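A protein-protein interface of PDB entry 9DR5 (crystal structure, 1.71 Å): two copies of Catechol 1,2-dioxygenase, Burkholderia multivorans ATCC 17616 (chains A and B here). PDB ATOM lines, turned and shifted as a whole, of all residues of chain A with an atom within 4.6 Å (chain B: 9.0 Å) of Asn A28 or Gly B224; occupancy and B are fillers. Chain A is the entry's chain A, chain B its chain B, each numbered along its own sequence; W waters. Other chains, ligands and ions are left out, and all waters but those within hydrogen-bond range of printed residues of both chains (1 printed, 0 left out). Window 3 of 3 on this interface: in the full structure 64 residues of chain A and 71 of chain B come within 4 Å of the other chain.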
ATOM      1  N   LYS A  24      31.842 -30.688   6.733  1.00  0.00           N
ATOM      2  CA  LYS A  24      30.882 -29.990   5.890  1.00  0.00           C
ATOM      3  C   LYS A  24      29.529 -29.900   6.573  1.00  0.00           C
ATOM      4  O   LYS A  24      28.858 -28.856   6.510  1.00  0.00           O
ATOM      5  CB  LYS A  24      30.756 -30.695   4.542  1.00  0.00           C
ATOM      6  CG  LYS A  24      31.905 -30.412   3.604  1.00  0.00           C
ATOM      7  CD  LYS A  24      31.804 -31.252   2.336  1.00  0.00           C
ATOM      8  CE  LYS A  24      33.154 -31.342   1.636  1.00  0.00           C
ATOM      9  NZ  LYS A  24      33.110 -32.180   0.401  1.00  0.00           N
ATOM     10  N   ALA A  25      29.106 -30.997   7.216  1.00  0.00           N
ATOM     11  CA  ALA A  25      27.834 -31.015   7.928  1.00  0.00           C
ATOM     12  C   ALA A  25      27.865 -30.093   9.131  1.00  0.00           C
ATOM     13  O   ALA A  25      26.920 -29.329   9.364  1.00  0.00           O
ATOM     14  CB  ALA A  25      27.502 -32.432   8.387  1.00  0.00           C
ATOM     15  N   ALA A  26      28.949 -30.158   9.910  1.00  0.00           N
ATOM     16  CA  ALA A  26      29.019 -29.391  11.145  1.00  0.00           C
ATOM     17  C   ALA A  26      28.964 -27.895  10.882  1.00  0.00           C
ATOM     18  O   ALA A  26      28.385 -27.152  11.680  1.00  0.00           O
ATOM     19  CB  ALA A  26      30.285 -29.754  11.917  1.00  0.00           C
ATOM     20  N   ALA A  27      29.537 -27.431   9.769  1.00  0.00           N
ATOM     21  CA  ALA A  27      29.482 -26.031   9.398  1.00  0.00           C
ATOM     22  C   ALA A  27      28.321 -25.699   8.461  1.00  0.00           C
ATOM     23  O   ALA A  27      28.160 -24.532   8.094  1.00  0.00           O
ATOM     24  CB  ALA A  27      30.808 -25.623   8.744  1.00  0.00           C
ATOM     25  N   ASN A  28      27.539 -26.700   8.059  1.00  0.00           N
ATOM     26  CA  ASN A  28      26.358 -26.534   7.207  1.00  0.00           C
ATOM     27  C   ASN A  28      26.693 -25.866   5.877  1.00  0.00           C
ATOM     28  O   ASN A  28      25.951 -25.014   5.388  1.00  0.00           O
ATOM     29  CB  ASN A  28      25.251 -25.759   7.928  1.00  0.00           C
ATOM     30  CG  ASN A  28      23.884 -25.995   7.309  1.00  0.00           C
ATOM     31  OD1 ASN A  28      23.631 -27.060   6.733  1.00  0.00           O
ATOM     32  ND2 ASN A  28      22.996 -25.006   7.415  1.00  0.00           N
ATOM     33  N   LEU A  29      27.795 -26.284   5.254  1.00  0.00           N
ATOM     34  CA  LEU A  29      28.190 -25.642   4.003  1.00  0.00           C
ATOM     35  C   LEU A  29      27.165 -25.865   2.900  1.00  0.00           C
ATOM     36  O   LEU A  29      26.996 -25.004   2.030  1.00  0.00           O
ATOM     37  CB  LEU A  29      29.549 -26.150   3.543  1.00  0.00           C
ATOM     38  CG  LEU A  29      30.750 -25.791   4.401  1.00  0.00           C
ATOM     39  CD1 LEU A  29      32.022 -26.025   3.610  1.00  0.00           C
ATOM     40  CD2 LEU A  29      30.684 -24.362   4.858  1.00  0.00           C
ATOM     41  N   ASN A  30      26.486 -27.010   2.900  1.00  0.00           N
ATOM     42  CA  ASN A  30      25.470 -27.308   1.897  1.00  0.00           C
ATOM     43  C   ASN A  30      24.058 -27.033   2.407  1.00  0.00           C
ATOM     44  O   ASN A  30      23.100 -27.664   1.947  1.00  0.00           O
ATOM     45  CB  ASN A  30      25.593 -28.759   1.436  1.00  0.00           C
ATOM     46  CG  ASN A  30      26.910 -29.038   0.744  1.00  0.00           C
ATOM     47  OD1 ASN A  30      27.312 -28.314  -0.170  1.00  0.00           O
ATOM     48  ND2 ASN A  30      27.602 -30.083   1.188  1.00  0.00           N
ATOM     49  N   GLY A  31      23.913 -26.107   3.358  1.00  0.00           N
ATOM     50  CA  GLY A  31      22.614 -25.770   3.897  1.00  0.00           C
ATOM     51  C   GLY A  31      21.903 -24.727   3.055  1.00  0.00           C
ATOM     52  O   GLY A  31      22.443 -24.184   2.092  1.00  0.00           O
ATOM     53  N   ARG A  39      29.614 -19.493   8.158  1.00  0.00           N
ATOM     54  CA  ARG A  39      29.840 -20.902   7.879  1.00  0.00           C
ATOM     55  C   ARG A  39      31.242 -21.129   7.338  1.00  0.00           C
ATOM     56  O   ARG A  39      31.899 -22.107   7.697  1.00  0.00           O
ATOM     57  CB  ARG A  39      28.797 -21.414   6.886  1.00  0.00           C
ATOM     58  CG  ARG A  39      27.364 -21.371   7.386  1.00  0.00           C
ATOM     59  CD  ARG A  39      26.426 -21.812   6.262  1.00  0.00           C
ATOM     60  NE  ARG A  39      25.022 -21.689   6.621  1.00  0.00           N
ATOM     61  CZ  ARG A  39      24.022 -21.957   5.794  1.00  0.00           C
ATOM     62  NH1 ARG A  39      24.245 -22.366   4.555  1.00  0.00           N
ATOM     63  NH2 ARG A  39      22.769 -21.803   6.220  1.00  0.00           N
ATOM     64  N   GLY B  85      28.211 -30.715  19.435  1.00  0.00           N
ATOM     65  CA  GLY B  85      27.416 -30.115  18.377  1.00  0.00           C
ATOM     66  C   GLY B  85      28.181 -29.769  17.109  1.00  0.00           C
ATOM     67  O   GLY B  85      27.599 -29.755  16.020  1.00  0.00           O
ATOM     68  N   ILE B  86      29.477 -29.474  17.206  1.00  0.00           N
ATOM     69  CA  ILE B  86      30.257 -29.240  15.991  1.00  0.00           C
ATOM     70  C   ILE B  86      31.105 -30.460  15.613  1.00  0.00           C
ATOM     71  O   ILE B  86      32.035 -30.346  14.810  1.00  0.00           O
ATOM     72  CB  ILE B  86      31.105 -27.957  16.055  1.00  0.00           C
ATOM     73  CG1 ILE B  86      31.752 -27.721  17.401  1.00  0.00           C
ATOM     74  CG2 ILE B  86      30.209 -26.777  15.670  1.00  0.00           C
ATOM     75  CD1 ILE B  86      32.815 -28.724  17.767  1.00  0.00           C
ATOM     76  N   GLN B 217      23.255 -23.485  21.038  1.00  0.00           N
ATOM     77  CA  GLN B 217      22.175 -23.204  20.109  1.00  0.00           C
ATOM     78  C   GLN B 217      22.380 -21.873  19.411  1.00  0.00           C
ATOM     79  O   GLN B 217      21.964 -21.708  18.259  1.00  0.00           O
ATOM     80  CB  GLN B 217      20.831 -23.221  20.839  1.00  0.00           C
ATOM     81  CG  GLN B 217      19.657 -23.161  19.906  1.00  0.00           C
ATOM     82  CD  GLN B 217      19.552 -24.402  19.065  1.00  0.00           C
ATOM     83  OE1 GLN B 217      19.535 -25.510  19.589  1.00  0.00           O
ATOM     84  NE2 GLN B 217      19.516 -24.229  17.752  1.00  0.00           N
ATOM     85  N   GLN B 218      23.027 -20.913  20.076  1.00  0.00           N
ATOM     86  CA  GLN B 218      23.295 -19.642  19.413  1.00  0.00           C
ATOM     87  C   GLN B 218      24.190 -19.856  18.201  1.00  0.00           C
ATOM     88  O   GLN B 218      23.940 -19.315  17.121  1.00  0.00           O
ATOM     89  CB  GLN B 218      23.942 -18.655  20.393  1.00  0.00           C
ATOM     90  CG  GLN B 218      24.166 -17.259  19.812  1.00  0.00           C
ATOM     91  CD  GLN B 218      24.854 -16.329  20.799  1.00  0.00           C
ATOM     92  OE1 GLN B 218      24.212 -15.547  21.493  1.00  0.00           O
ATOM     93  NE2 GLN B 218      26.158 -16.428  20.874  1.00  0.00           N
ATOM     94  N   LEU B 219      25.241 -20.651  18.363  1.00  0.00           N
ATOM     95  CA  LEU B 219      26.136 -20.902  17.237  1.00  0.00           C
ATOM     96  C   LEU B 219      25.425 -21.716  16.166  1.00  0.00           C
ATOM     97  O   LEU B 219      25.518 -21.401  14.976  1.00  0.00           O
ATOM     98  CB  LEU B 219      27.403 -21.605  17.728  1.00  0.00           C
ATOM     99  CG  LEU B 219      28.439 -22.023  16.677  1.00  0.00           C
ATOM    100  CD1 LEU B 219      29.841 -21.950  17.268  1.00  0.00           C
ATOM    101  CD2 LEU B 219      28.145 -23.454  16.205  1.00  0.00           C
ATOM    102  N   LEU B 220      24.660 -22.734  16.575  1.00  0.00           N
ATOM    103  CA  LEU B 220      23.917 -23.517  15.596  1.00  0.00           C
ATOM    104  C   LEU B 220      22.933 -22.634  14.837  1.00  0.00           C
ATOM    105  O   LEU B 220      22.786 -22.763  13.617  1.00  0.00           O
ATOM    106  CB  LEU B 220      23.192 -24.680  16.283  1.00  0.00           C
ATOM    107  CG  LEU B 220      24.086 -25.701  16.978  1.00  0.00           C
ATOM    108  CD1 LEU B 220      23.249 -26.640  17.839  1.00  0.00           C
ATOM    109  CD2 LEU B 220      24.902 -26.501  15.940  1.00  0.00           C
ATOM    110  N   ASN B 221      22.255 -21.726  15.542  1.00  0.00           N
ATOM    111  CA  ASN B 221      21.357 -20.793  14.864  1.00  0.00           C
ATOM    112  C   ASN B 221      22.105 -19.993  13.810  1.00  0.00           C
ATOM    113  O   ASN B 221      21.601 -19.781  12.699  1.00  0.00           O
ATOM    114  CB  ASN B 221      20.706 -19.836  15.874  1.00  0.00           C
ATOM    115  CG  ASN B 221      19.646 -20.512  16.722  1.00  0.00           C
ATOM    116  OD1 ASN B 221      19.206 -21.616  16.418  1.00  0.00           O
ATOM    117  ND2 ASN B 221      19.227 -19.843  17.791  1.00  0.00           N
ATOM    118  N   GLY B 222      23.308 -19.526  14.143  1.00  0.00           N
ATOM    119  CA  GLY B 222      24.097 -18.782  13.179  1.00  0.00           C
ATOM    120  C   GLY B 222      24.473 -19.600  11.959  1.00  0.00           C
ATOM    121  O   GLY B 222      24.605 -19.051  10.862  1.00  0.00           O
ATOM    122  N   LEU B 223      24.656 -20.916  12.130  1.00  0.00           N
ATOM    123  CA  LEU B 223      24.949 -21.803  11.011  1.00  0.00           C
ATOM    124  C   LEU B 223      23.709 -22.241  10.253  1.00  0.00           C
ATOM    125  O   LEU B 223      23.845 -22.837   9.181  1.00  0.00           O
ATOM    126  CB  LEU B 223      25.676 -23.060  11.501  1.00  0.00           C
ATOM    127  CG  LEU B 223      27.032 -22.818  12.159  1.00  0.00           C
ATOM    128  CD1 LEU B 223      27.575 -24.093  12.796  1.00  0.00           C
ATOM    129  CD2 LEU B 223      28.001 -22.291  11.138  1.00  0.00           C
ATOM    130  N   GLY B 224      22.514 -21.989  10.787  1.00  0.00           N
ATOM    131  CA  GLY B 224      21.306 -22.502  10.174  1.00  0.00           C
ATOM    132  C   GLY B 224      20.995 -23.932  10.545  1.00  0.00           C
ATOM    133  O   GLY B 224      20.258 -24.604   9.816  1.00  0.00           O
ATOM    134  N   ARG B 225      21.543 -24.427  11.651  1.00  0.00           N
ATOM    135  CA  ARG B 225      21.389 -25.816  12.056  1.00  0.00           C
ATOM    136  C   ARG B 225      20.465 -25.936  13.260  1.00  0.00           C
ATOM    137  O   ARG B 225      20.413 -25.052  14.122  1.00  0.00           O
ATOM    138  CB  ARG B 225      22.745 -26.447  12.417  1.00  0.00           C
ATOM    139  CG  ARG B 225      23.692 -26.639  11.241  1.00  0.00           C
ATOM    140  CD  ARG B 225      24.993 -27.265  11.718  1.00  0.00           C
ATOM    141  NE  ARG B 225      24.735 -28.459  12.514  1.00  0.00           N
ATOM    142  CZ  ARG B 225      25.526 -28.917  13.473  1.00  0.00           C
ATOM    143  NH1 ARG B 225      26.728 -28.417  13.672  1.00  0.00           N
ATOM    144  NH2 ARG B 225      25.065 -29.846  14.301  1.00  0.00           N
ATOM    145  N   HIS B 226      19.765 -27.062  13.338  1.00  0.00           N
ATOM    146  CA  HIS B 226      19.006 -27.356  14.541  1.00  0.00           C
ATOM    147  C   HIS B 226      19.907 -27.985  15.598  1.00  0.00           C
ATOM    148  O   HIS B 226      21.018 -28.455  15.316  1.00  0.00           O
ATOM    149  CB  HIS B 226      17.826 -28.292  14.236  1.00  0.00           C
ATOM    150  CG  HIS B 226      18.230 -29.707  13.949  1.00  0.00           C
ATOM    151  ND1 HIS B 226      18.668 -30.574  14.928  1.00  0.00           N
ATOM    152  CD2 HIS B 226      18.245 -30.412  12.792  1.00  0.00           C
ATOM    153  CE1 HIS B 226      18.949 -31.746  14.387  1.00  0.00           C
ATOM    154  NE2 HIS B 226      18.700 -31.673  13.090  1.00  0.00           N
ATOM    155  N   GLY B 227      19.414 -27.971  16.837  1.00  0.00           N
ATOM    156  CA  GLY B 227      20.145 -28.501  17.968  1.00  0.00           C
ATOM    157  C   GLY B 227      19.438 -29.660  18.643  1.00  0.00           C
ATOM    158  O   GLY B 227      19.477 -29.800  19.867  1.00  0.00           O
ATOM    159  N   ASP B 259      19.664 -37.510  11.664  1.00  0.00           N
ATOM    160  CA  ASP B 259      19.864 -36.061  11.633  1.00  0.00           C
ATOM    161  C   ASP B 259      20.146 -35.546  13.046  1.00  0.00           C
ATOM    162  O   ASP B 259      19.642 -34.497  13.464  1.00  0.00           O
ATOM    163  CB  ASP B 259      18.664 -35.346  11.012  1.00  0.00           C
ATOM    164  CG  ASP B 259      18.990 -33.920  10.575  1.00  0.00           C
ATOM    165  OD1 ASP B 259      20.185 -33.581  10.463  1.00  0.00           O
ATOM    166  OD2 ASP B 259      18.045 -33.136  10.343  1.00  0.00           O
ATOM    167  N   TYR B 263      25.771 -36.101  15.687  1.00  0.00           N
ATOM    168  CA  TYR B 263      26.381 -37.020  14.719  1.00  0.00           C
ATOM    169  C   TYR B 263      26.728 -38.388  15.314  1.00  0.00           C
ATOM    170  O   TYR B 263      27.713 -39.018  14.923  1.00  0.00           O
ATOM    171  CB  TYR B 263      27.630 -36.380  14.103  1.00  0.00           C
ATOM    172  CG  TYR B 263      27.341 -35.025  13.480  1.00  0.00           C
ATOM    173  CD1 TYR B 263      26.550 -34.928  12.340  1.00  0.00           C
ATOM    174  CD2 TYR B 263      27.830 -33.855  14.042  1.00  0.00           C
ATOM    175  CE1 TYR B 263      26.253 -33.708  11.773  1.00  0.00           C
ATOM    176  CE2 TYR B 263      27.551 -32.620  13.477  1.00  0.00           C
ATOM    177  CZ  TYR B 263      26.763 -32.551  12.337  1.00  0.00           C
ATOM    178  OH  TYR B 263      26.466 -31.349  11.764  1.00  0.00           O
HETATM  179  O   HOH W   1      23.473 -19.539   8.322  1.00  0.00           O
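The backbone carbonyl oxygen (O) of Ala A25 lies within hydrogen-bond range of the side-chain hydroxyl (OH) of Tyr B263.
The backbone carbonyl oxygen of Ala A26 lies within hydrogen-bond range of the guanidinium group of Arg B225 (2.9 Å).
The side-chain hydroxyl (OH) of Tyr B263 lies close to the backbone NH (N) of Ala A26, 3.3 Å away.
O of Leu B223 is in hydrogen-bond range of ND2 of Asn A28 (2.9 Å).
The backbone carbonyl oxygen of Leu B223 is in hydrogen-bond range of the guanidinium group of Arg A39 (3.0 Å).
The guanidinium group (NH1) of Arg A39 sits at hydrogen-bond distance from the backbone carbonyl oxygen (O) of Asn A28 (3.3 Å).
The backbone carbonyl oxygen (O) of Gly B85 lies within hydrogen-bond range of the guanidinium group (NH1) of Arg B225 (2.8 Å).
O of Leu B220 sits at hydrogen-bond distance from N of Arg B225, 2.9 Å away.
The guanidinium group (NH2) of Arg B225 lies close to the side-chain hydroxyl (OH) of Tyr B263, at 3.3 Å.
Among the printed residues, pairs that only touch across the chains: Ala A25 with Arg B225, Ala A26 with Ile B86, Ala A26 with Leu B223, Ala A27 with Leu B223, Asn A28 with Gly B224 and Asn A28 with Arg B225.
Of chain B, only Leu B223, Gly B224 and Arg B225 come within 4 Å of Asn A28.
Of chain A, only Asn A28 comes within 4 Å of Gly B224.
Printed residues of chain B within 4 Å of Ala A25: Arg B225 (3.7 Å) and Tyr B263 (3.2 Å).
Printed residues of chain A within 4 Å of Tyr B263: Ala A25 (3.2 Å) and Ala A26 (3.3 Å).
Printed residues of chain A within 4 Å of Arg B225: Ala A25 (3.7 Å), Ala A26 (2.9 Å) and Asn A28 (3.8 Å).
Asp B259 touches none of the printed residues of chain A.
The nearest residue of chain B that does not touch Asn A28 is Tyr B263 (6.0 Å).
The nearest printed residue of chain B that does not touch Ala A25 is Leu B223 (6.3 Å).
Of the 9 printed residues of chain A, 5 touch a printed residue of chain B.
Hydrophobic or aromatic side chains of chain A that line the printed part of chain B: Ala A25 and Ala A26.
Of the 15 printed residues of chain B, 5 touch a printed residue of chain A.
Hydrophobic or aromatic side chains of chain B within 4 Å of the printed part of chain A: Leu B223 and Tyr B263.
Among the printed residues, 11 pairs touch across the chains.
No position is printed for both chains.
Water W1 lies within hydrogen-bond range of the backbone carbonyl oxygen of Gly B222, the guanidinium group of Arg A39 and the backbone carbonyl oxygen of Leu B223.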
